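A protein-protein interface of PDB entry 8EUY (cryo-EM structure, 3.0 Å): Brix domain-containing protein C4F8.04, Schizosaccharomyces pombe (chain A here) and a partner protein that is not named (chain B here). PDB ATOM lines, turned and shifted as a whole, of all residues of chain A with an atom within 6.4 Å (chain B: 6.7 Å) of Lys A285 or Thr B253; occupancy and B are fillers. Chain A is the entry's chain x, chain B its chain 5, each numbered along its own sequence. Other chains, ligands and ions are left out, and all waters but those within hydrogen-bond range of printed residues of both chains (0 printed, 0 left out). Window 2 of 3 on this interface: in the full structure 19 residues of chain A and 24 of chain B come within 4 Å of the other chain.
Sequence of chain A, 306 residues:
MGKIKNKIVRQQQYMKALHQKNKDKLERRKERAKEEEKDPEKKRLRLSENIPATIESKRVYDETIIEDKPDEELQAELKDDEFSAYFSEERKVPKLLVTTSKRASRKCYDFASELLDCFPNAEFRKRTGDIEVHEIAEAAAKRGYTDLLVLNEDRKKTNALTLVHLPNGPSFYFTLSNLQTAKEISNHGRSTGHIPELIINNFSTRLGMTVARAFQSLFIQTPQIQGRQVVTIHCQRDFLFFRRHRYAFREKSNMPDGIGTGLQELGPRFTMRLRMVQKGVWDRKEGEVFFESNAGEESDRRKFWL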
ATOM      1  N   GLN A 278      -2.474 -31.007   8.754  1.00  0.00           N
ATOM      2  CA  GLN A 278      -2.531 -29.587   8.451  1.00  0.00           C
ATOM      3  C   GLN A 278      -3.975 -29.127   8.352  1.00  0.00           C
ATOM      4  O   GLN A 278      -4.855 -29.876   7.921  1.00  0.00           O
ATOM      5  CB  GLN A 278      -1.804 -29.261   7.144  1.00  0.00           C
ATOM      6  CG  GLN A 278      -0.308 -29.471   7.193  1.00  0.00           C
ATOM      7  CD  GLN A 278       0.410 -28.728   6.095  1.00  0.00           C
ATOM      8  OE1 GLN A 278      -0.112 -28.570   4.996  1.00  0.00           O
ATOM      9  NE2 GLN A 278       1.620 -28.270   6.384  1.00  0.00           N
ATOM     10  N   ASP A 283       0.237 -28.153   2.197  1.00  0.00           N
ATOM     11  CA  ASP A 283       1.298 -27.277   1.706  1.00  0.00           C
ATOM     12  C   ASP A 283       2.447 -27.391   2.703  1.00  0.00           C
ATOM     13  O   ASP A 283       2.368 -26.838   3.802  1.00  0.00           O
ATOM     14  CB  ASP A 283       0.815 -25.845   1.564  1.00  0.00           C
ATOM     15  CG  ASP A 283       1.778 -24.982   0.782  1.00  0.00           C
ATOM     16  OD1 ASP A 283       2.795 -25.516   0.293  1.00  0.00           O
ATOM     17  OD2 ASP A 283       1.518 -23.770   0.647  1.00  0.00           O
ATOM     18  N   ARG A 284       3.500 -28.113   2.317  1.00  0.00           N
ATOM     19  CA  ARG A 284       4.580 -28.395   3.254  1.00  0.00           C
ATOM     20  C   ARG A 284       5.299 -27.136   3.711  1.00  0.00           C
ATOM     21  O   ARG A 284       5.904 -27.140   4.787  1.00  0.00           O
ATOM     22  CB  ARG A 284       5.577 -29.371   2.631  1.00  0.00           C
ATOM     23  CG  ARG A 284       6.136 -28.934   1.293  1.00  0.00           C
ATOM     24  CD  ARG A 284       7.460 -29.619   1.006  1.00  0.00           C
ATOM     25  NE  ARG A 284       8.409 -29.417   2.092  1.00  0.00           N
ATOM     26  CZ  ARG A 284       9.255 -28.399   2.166  1.00  0.00           C
ATOM     27  NH1 ARG A 284       9.320 -27.484   1.213  1.00  0.00           N
ATOM     28  NH2 ARG A 284      10.057 -28.297   3.221  1.00  0.00           N
ATOM     29  N   LYS A 285       5.242 -26.059   2.931  1.00  0.00           N
ATOM     30  CA  LYS A 285       5.949 -24.833   3.284  1.00  0.00           C
ATOM     31  C   LYS A 285       5.047 -23.854   4.031  1.00  0.00           C
ATOM     32  O   LYS A 285       5.365 -23.434   5.146  1.00  0.00           O
ATOM     33  CB  LYS A 285       6.523 -24.182   2.021  1.00  0.00           C
ATOM     34  CG  LYS A 285       7.510 -23.054   2.291  1.00  0.00           C
ATOM     35  CD  LYS A 285       7.759 -22.227   1.040  1.00  0.00           C
ATOM     36  CE  LYS A 285       8.358 -23.077  -0.069  1.00  0.00           C
ATOM     37  NZ  LYS A 285       8.488 -22.329  -1.347  1.00  0.00           N
ATOM     38  N   GLU A 286       3.917 -23.490   3.428  1.00  0.00           N
ATOM     39  CA  GLU A 286       3.039 -22.459   3.960  1.00  0.00           C
ATOM     40  C   GLU A 286       1.826 -23.024   4.687  1.00  0.00           C
ATOM     41  O   GLU A 286       0.888 -22.278   4.975  1.00  0.00           O
ATOM     42  CB  GLU A 286       2.584 -21.528   2.835  1.00  0.00           C
ATOM     43  CG  GLU A 286       3.618 -21.324   1.742  1.00  0.00           C
ATOM     44  CD  GLU A 286       3.171 -20.333   0.681  1.00  0.00           C
ATOM     45  OE1 GLU A 286       2.252 -19.533   0.957  1.00  0.00           O
ATOM     46  OE2 GLU A 286       3.736 -20.356  -0.432  1.00  0.00           O
ATOM     47  N   GLY A 287       1.818 -24.320   4.985  1.00  0.00           N
ATOM     48  CA  GLY A 287       0.684 -24.911   5.658  1.00  0.00           C
ATOM     49  C   GLY A 287       0.647 -24.605   7.142  1.00  0.00           C
ATOM     50  O   GLY A 287       1.646 -24.249   7.762  1.00  0.00           O
ATOM     51  N   ARG B 195       8.007 -10.567  -2.838  1.00  0.00           N
ATOM     52  CA  ARG B 195       6.564 -10.411  -2.777  1.00  0.00           C
ATOM     53  C   ARG B 195       6.144  -9.773  -1.459  1.00  0.00           C
ATOM     54  O   ARG B 195       6.824  -9.895  -0.438  1.00  0.00           O
ATOM     55  CB  ARG B 195       5.881 -11.763  -2.955  1.00  0.00           C
ATOM     56  CG  ARG B 195       5.995 -12.322  -4.357  1.00  0.00           C
ATOM     57  CD  ARG B 195       5.687 -13.805  -4.383  1.00  0.00           C
ATOM     58  NE  ARG B 195       6.686 -14.568  -3.646  1.00  0.00           N
ATOM     59  CZ  ARG B 195       6.662 -15.884  -3.497  1.00  0.00           C
ATOM     60  NH1 ARG B 195       5.699 -16.622  -4.022  1.00  0.00           N
ATOM     61  NH2 ARG B 195       7.628 -16.475  -2.803  1.00  0.00           N
ATOM     62  N   HIS B 230       3.762 -12.907   5.204  1.00  0.00           N
ATOM     63  CA  HIS B 230       3.429 -14.287   4.878  1.00  0.00           C
ATOM     64  C   HIS B 230       4.645 -15.098   4.456  1.00  0.00           C
ATOM     65  O   HIS B 230       4.572 -16.328   4.424  1.00  0.00           O
ATOM     66  CB  HIS B 230       2.376 -14.302   3.769  1.00  0.00           C
ATOM     67  CG  HIS B 230       2.036 -15.667   3.262  1.00  0.00           C
ATOM     68  ND1 HIS B 230       1.277 -16.562   3.983  1.00  0.00           N
ATOM     69  CD2 HIS B 230       2.343 -16.286   2.098  1.00  0.00           C
ATOM     70  CE1 HIS B 230       1.135 -17.676   3.287  1.00  0.00           C
ATOM     71  NE2 HIS B 230       1.772 -17.534   2.140  1.00  0.00           N
ATOM     72  N   TYR B 231       5.758 -14.443   4.135  1.00  0.00           N
ATOM     73  CA  TYR B 231       6.968 -15.124   3.709  1.00  0.00           C
ATOM     74  C   TYR B 231       8.026 -15.154   4.803  1.00  0.00           C
ATOM     75  O   TYR B 231       9.208 -15.356   4.514  1.00  0.00           O
ATOM     76  CB  TYR B 231       7.505 -14.474   2.438  1.00  0.00           C
ATOM     77  CG  TYR B 231       6.428 -14.287   1.396  1.00  0.00           C
ATOM     78  CD1 TYR B 231       6.068 -15.323   0.552  1.00  0.00           C
ATOM     79  CD2 TYR B 231       5.755 -13.081   1.274  1.00  0.00           C
ATOM     80  CE1 TYR B 231       5.078 -15.162  -0.390  1.00  0.00           C
ATOM     81  CE2 TYR B 231       4.763 -12.912   0.336  1.00  0.00           C
ATOM     82  CZ  TYR B 231       4.430 -13.954  -0.493  1.00  0.00           C
ATOM     83  OH  TYR B 231       3.442 -13.786  -1.432  1.00  0.00           O
ATOM     84  N   GLY B 232       7.618 -14.953   6.050  1.00  0.00           N
ATOM     85  CA  GLY B 232       8.489 -15.125   7.197  1.00  0.00           C
ATOM     86  C   GLY B 232       9.651 -14.166   7.294  1.00  0.00           C
ATOM     87  O   GLY B 232      10.762 -14.584   7.639  1.00  0.00           O
ATOM     88  N   ASP B 250      14.878 -12.592   7.889  1.00  0.00           N
ATOM     89  CA  ASP B 250      14.141 -13.793   7.496  1.00  0.00           C
ATOM     90  C   ASP B 250      14.059 -14.700   8.718  1.00  0.00           C
ATOM     91  O   ASP B 250      14.795 -15.677   8.870  1.00  0.00           O
ATOM     92  CB  ASP B 250      14.812 -14.486   6.319  1.00  0.00           C
ATOM     93  CG  ASP B 250      15.084 -13.544   5.165  1.00  0.00           C
ATOM     94  OD1 ASP B 250      14.476 -12.455   5.127  1.00  0.00           O
ATOM     95  OD2 ASP B 250      15.908 -13.892   4.295  1.00  0.00           O
ATOM     96  N   VAL B 251      13.132 -14.353   9.615  1.00  0.00           N
ATOM     97  CA  VAL B 251      13.052 -15.003  10.921  1.00  0.00           C
ATOM     98  C   VAL B 251      12.409 -16.377  10.877  1.00  0.00           C
ATOM     99  O   VAL B 251      12.533 -17.134  11.848  1.00  0.00           O
ATOM    100  CB  VAL B 251      12.274 -14.117  11.909  1.00  0.00           C
ATOM    101  CG1 VAL B 251      13.129 -12.942  12.344  1.00  0.00           C
ATOM    102  CG2 VAL B 251      10.981 -13.637  11.279  1.00  0.00           C
ATOM    103  N   SER B 252      11.727 -16.727   9.791  1.00  0.00           N
ATOM    104  CA  SER B 252      11.065 -18.019   9.719  1.00  0.00           C
ATOM    105  C   SER B 252      10.872 -18.405   8.262  1.00  0.00           C
ATOM    106  O   SER B 252      10.833 -17.555   7.372  1.00  0.00           O
ATOM    107  CB  SER B 252       9.720 -17.999  10.450  1.00  0.00           C
ATOM    108  OG  SER B 252       8.971 -19.162  10.161  1.00  0.00           O
ATOM    109  N   THR B 253      10.754 -19.709   8.035  1.00  0.00           N
ATOM    110  CA  THR B 253      10.442 -20.257   6.725  1.00  0.00           C
ATOM    111  C   THR B 253       8.960 -20.556   6.559  1.00  0.00           C
ATOM    112  O   THR B 253       8.555 -21.078   5.518  1.00  0.00           O
ATOM    113  CB  THR B 253      11.260 -21.525   6.477  1.00  0.00           C
ATOM    114  OG1 THR B 253      10.878 -22.105   5.226  1.00  0.00           O
ATOM    115  CG2 THR B 253      11.026 -22.526   7.592  1.00  0.00           C
ATOM    116  N   SER B 254       8.147 -20.237   7.563  1.00  0.00           N
ATOM    117  CA  SER B 254       6.706 -20.391   7.547  1.00  0.00           C
ATOM    118  C   SER B 254       6.045 -19.023   7.659  1.00  0.00           C
ATOM    119  O   SER B 254       6.646 -18.087   8.194  1.00  0.00           O
ATOM    120  CB  SER B 254       6.237 -21.283   8.702  1.00  0.00           C
ATOM    121  OG  SER B 254       4.934 -21.784   8.466  1.00  0.00           O
ATOM    122  N   PRO B 255       4.829 -18.866   7.139  1.00  0.00           N
ATOM    123  CA  PRO B 255       4.130 -17.587   7.295  1.00  0.00           C
ATOM    124  C   PRO B 255       3.983 -17.205   8.759  1.00  0.00           C
ATOM    125  O   PRO B 255       3.668 -18.036   9.610  1.00  0.00           O
ATOM    126  CB  PRO B 255       2.766 -17.843   6.641  1.00  0.00           C
ATOM    127  CG  PRO B 255       2.758 -19.281   6.234  1.00  0.00           C
ATOM    128  CD  PRO B 255       4.161 -19.739   6.167  1.00  0.00           C
ATOM    129  N   ASP B 272       4.713 -18.081  14.060  1.00  0.00           N
ATOM    130  CA  ASP B 272       4.449 -18.498  12.690  1.00  0.00           C
ATOM    131  C   ASP B 272       3.434 -19.638  12.678  1.00  0.00           C
ATOM    132  O   ASP B 272       2.953 -20.085  13.720  1.00  0.00           O
ATOM    133  CB  ASP B 272       5.745 -18.906  11.985  1.00  0.00           C
ATOM    134  CG  ASP B 272       6.369 -20.143  12.585  1.00  0.00           C
ATOM    135  OD1 ASP B 272       6.065 -20.450  13.753  1.00  0.00           O
ATOM    136  OD2 ASP B 272       7.164 -20.812  11.894  1.00  0.00           O
ATOM    137  N   LYS B 273       3.113 -20.108  11.473  1.00  0.00           N
ATOM    138  CA  LYS B 273       2.144 -21.183  11.301  1.00  0.00           C
ATOM    139  C   LYS B 273       2.717 -22.562  11.596  1.00  0.00           C
ATOM    140  O   LYS B 273       1.955 -23.529  11.645  1.00  0.00           O
ATOM    141  CB  LYS B 273       1.584 -21.166   9.879  1.00  0.00           C
ATOM    142  CG  LYS B 273       0.719 -19.967   9.555  1.00  0.00           C
ATOM    143  CD  LYS B 273      -0.084 -20.224   8.295  1.00  0.00           C
ATOM    144  CE  LYS B 273      -1.070 -19.111   8.020  1.00  0.00           C
ATOM    145  NZ  LYS B 273      -1.617 -19.210   6.640  1.00  0.00           N
ATOM    146  N   ARG B 274       4.032 -22.678  11.782  1.00  0.00           N
ATOM    147  CA  ARG B 274       4.669 -23.954  12.083  1.00  0.00           C
ATOM    148  C   ARG B 274       4.792 -24.205  13.578  1.00  0.00           C
ATOM    149  O   ARG B 274       5.689 -24.945  14.002  1.00  0.00           O
ATOM    150  CB  ARG B 274       6.045 -24.026  11.423  1.00  0.00           C
ATOM    151  CG  ARG B 274       6.085 -24.822  10.133  1.00  0.00           C
ATOM    152  CD  ARG B 274       6.050 -26.318  10.408  1.00  0.00           C
ATOM    153  NE  ARG B 274       6.339 -27.121   9.224  1.00  0.00           N
ATOM    154  CZ  ARG B 274       5.540 -27.233   8.169  1.00  0.00           C
ATOM    155  NH1 ARG B 274       4.391 -26.582   8.095  1.00  0.00           N
ATOM    156  NH2 ARG B 274       5.907 -28.018   7.161  1.00  0.00           N
ATOM    157  N   GLN B 276       5.692 -22.250  16.160  1.00  0.00           N
ATOM    158  CA  GLN B 276       6.954 -21.760  16.699  1.00  0.00           C
ATOM    159  C   GLN B 276       6.782 -20.312  17.127  1.00  0.00           C
ATOM    160  O   GLN B 276       6.504 -19.444  16.295  1.00  0.00           O
ATOM    161  CB  GLN B 276       8.077 -21.896  15.667  1.00  0.00           C
ATOM    162  CG  GLN B 276       9.264 -20.983  15.889  1.00  0.00           C
ATOM    163  CD  GLN B 276      10.264 -21.067  14.756  1.00  0.00           C
ATOM    164  OE1 GLN B 276      10.473 -22.132  14.176  1.00  0.00           O
ATOM    165  NE2 GLN B 276      10.884 -19.939  14.427  1.00  0.00           N
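O of Arg A284 is in hydrogen-bond range of NH2 of Arg B274 (2.5 Å). The side-chain carboxylate of Glu A286 lies close to a ring nitrogen (NE2) of His B230, 2.4 Å away.
N of Asp A283 is in hydrogen-bond range of OE1 of Gln A278 (2.9 Å). The backbone NH of Ser B254 lies within hydrogen-bond range of the side-chain hydroxyl of Ser B252, 2.9 Å away. The backbone carbonyl oxygen (O) of Pro B255 sits at hydrogen-bond distance from the backbone NH (N) of Lys B273 (2.8 Å).
Gln A278 touches Arg B274 (NE2 to NH1, 3.7 Å). Lys A285 touches Thr B253. OG of Ser B254 touches O of Lys A285, 3.7 Å away. Glu A286 touches Pro B255 (CA to CD, 3.7 Å). Lys B273 touches Gly A287. O of Gly A287 touches NH1 of Arg B274, 3.6 Å away.
Printed residues of chain B within 4 Å of Gln A278: Arg B274. Printed residues of chain B within 4 Å of Gly A287: Lys B273 and Arg B274. Arg B195 touches none of the printed residues of chain A. Of chain A, only Lys A285 (3.9 Å) comes within 4 Å of Thr B253. Of the printed residues of chain A, Pro B255 touches Glu A286 (3.7 Å). Of the printed residues of chain A, Lys B273 touches Gly A287 (3.7 Å). Printed residues of chain A within 4 Å of Arg B274: Gln A278, Arg A284 and Gly A287. Gln B276 touches none of the printed residues of chain A. The nearest residue of chain A that does not touch Thr B253 is Glu A286 (5.6 Å). The nearest printed residue of chain B that does not touch Glu A286 is Lys B273 (4.02 Å).
Of the 6 printed residues of chain A, 5 touch a printed residue of chain B. Along chain B the printed residues that touch a printed residue of chain A span positions 230 to 274. Among the printed residues, 8 pairs touch across the chains. Among the printed residues, no Asp or Glu carboxylate lies within 4 Å of a Lys or Arg side-chain nitrogen of the other chain.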
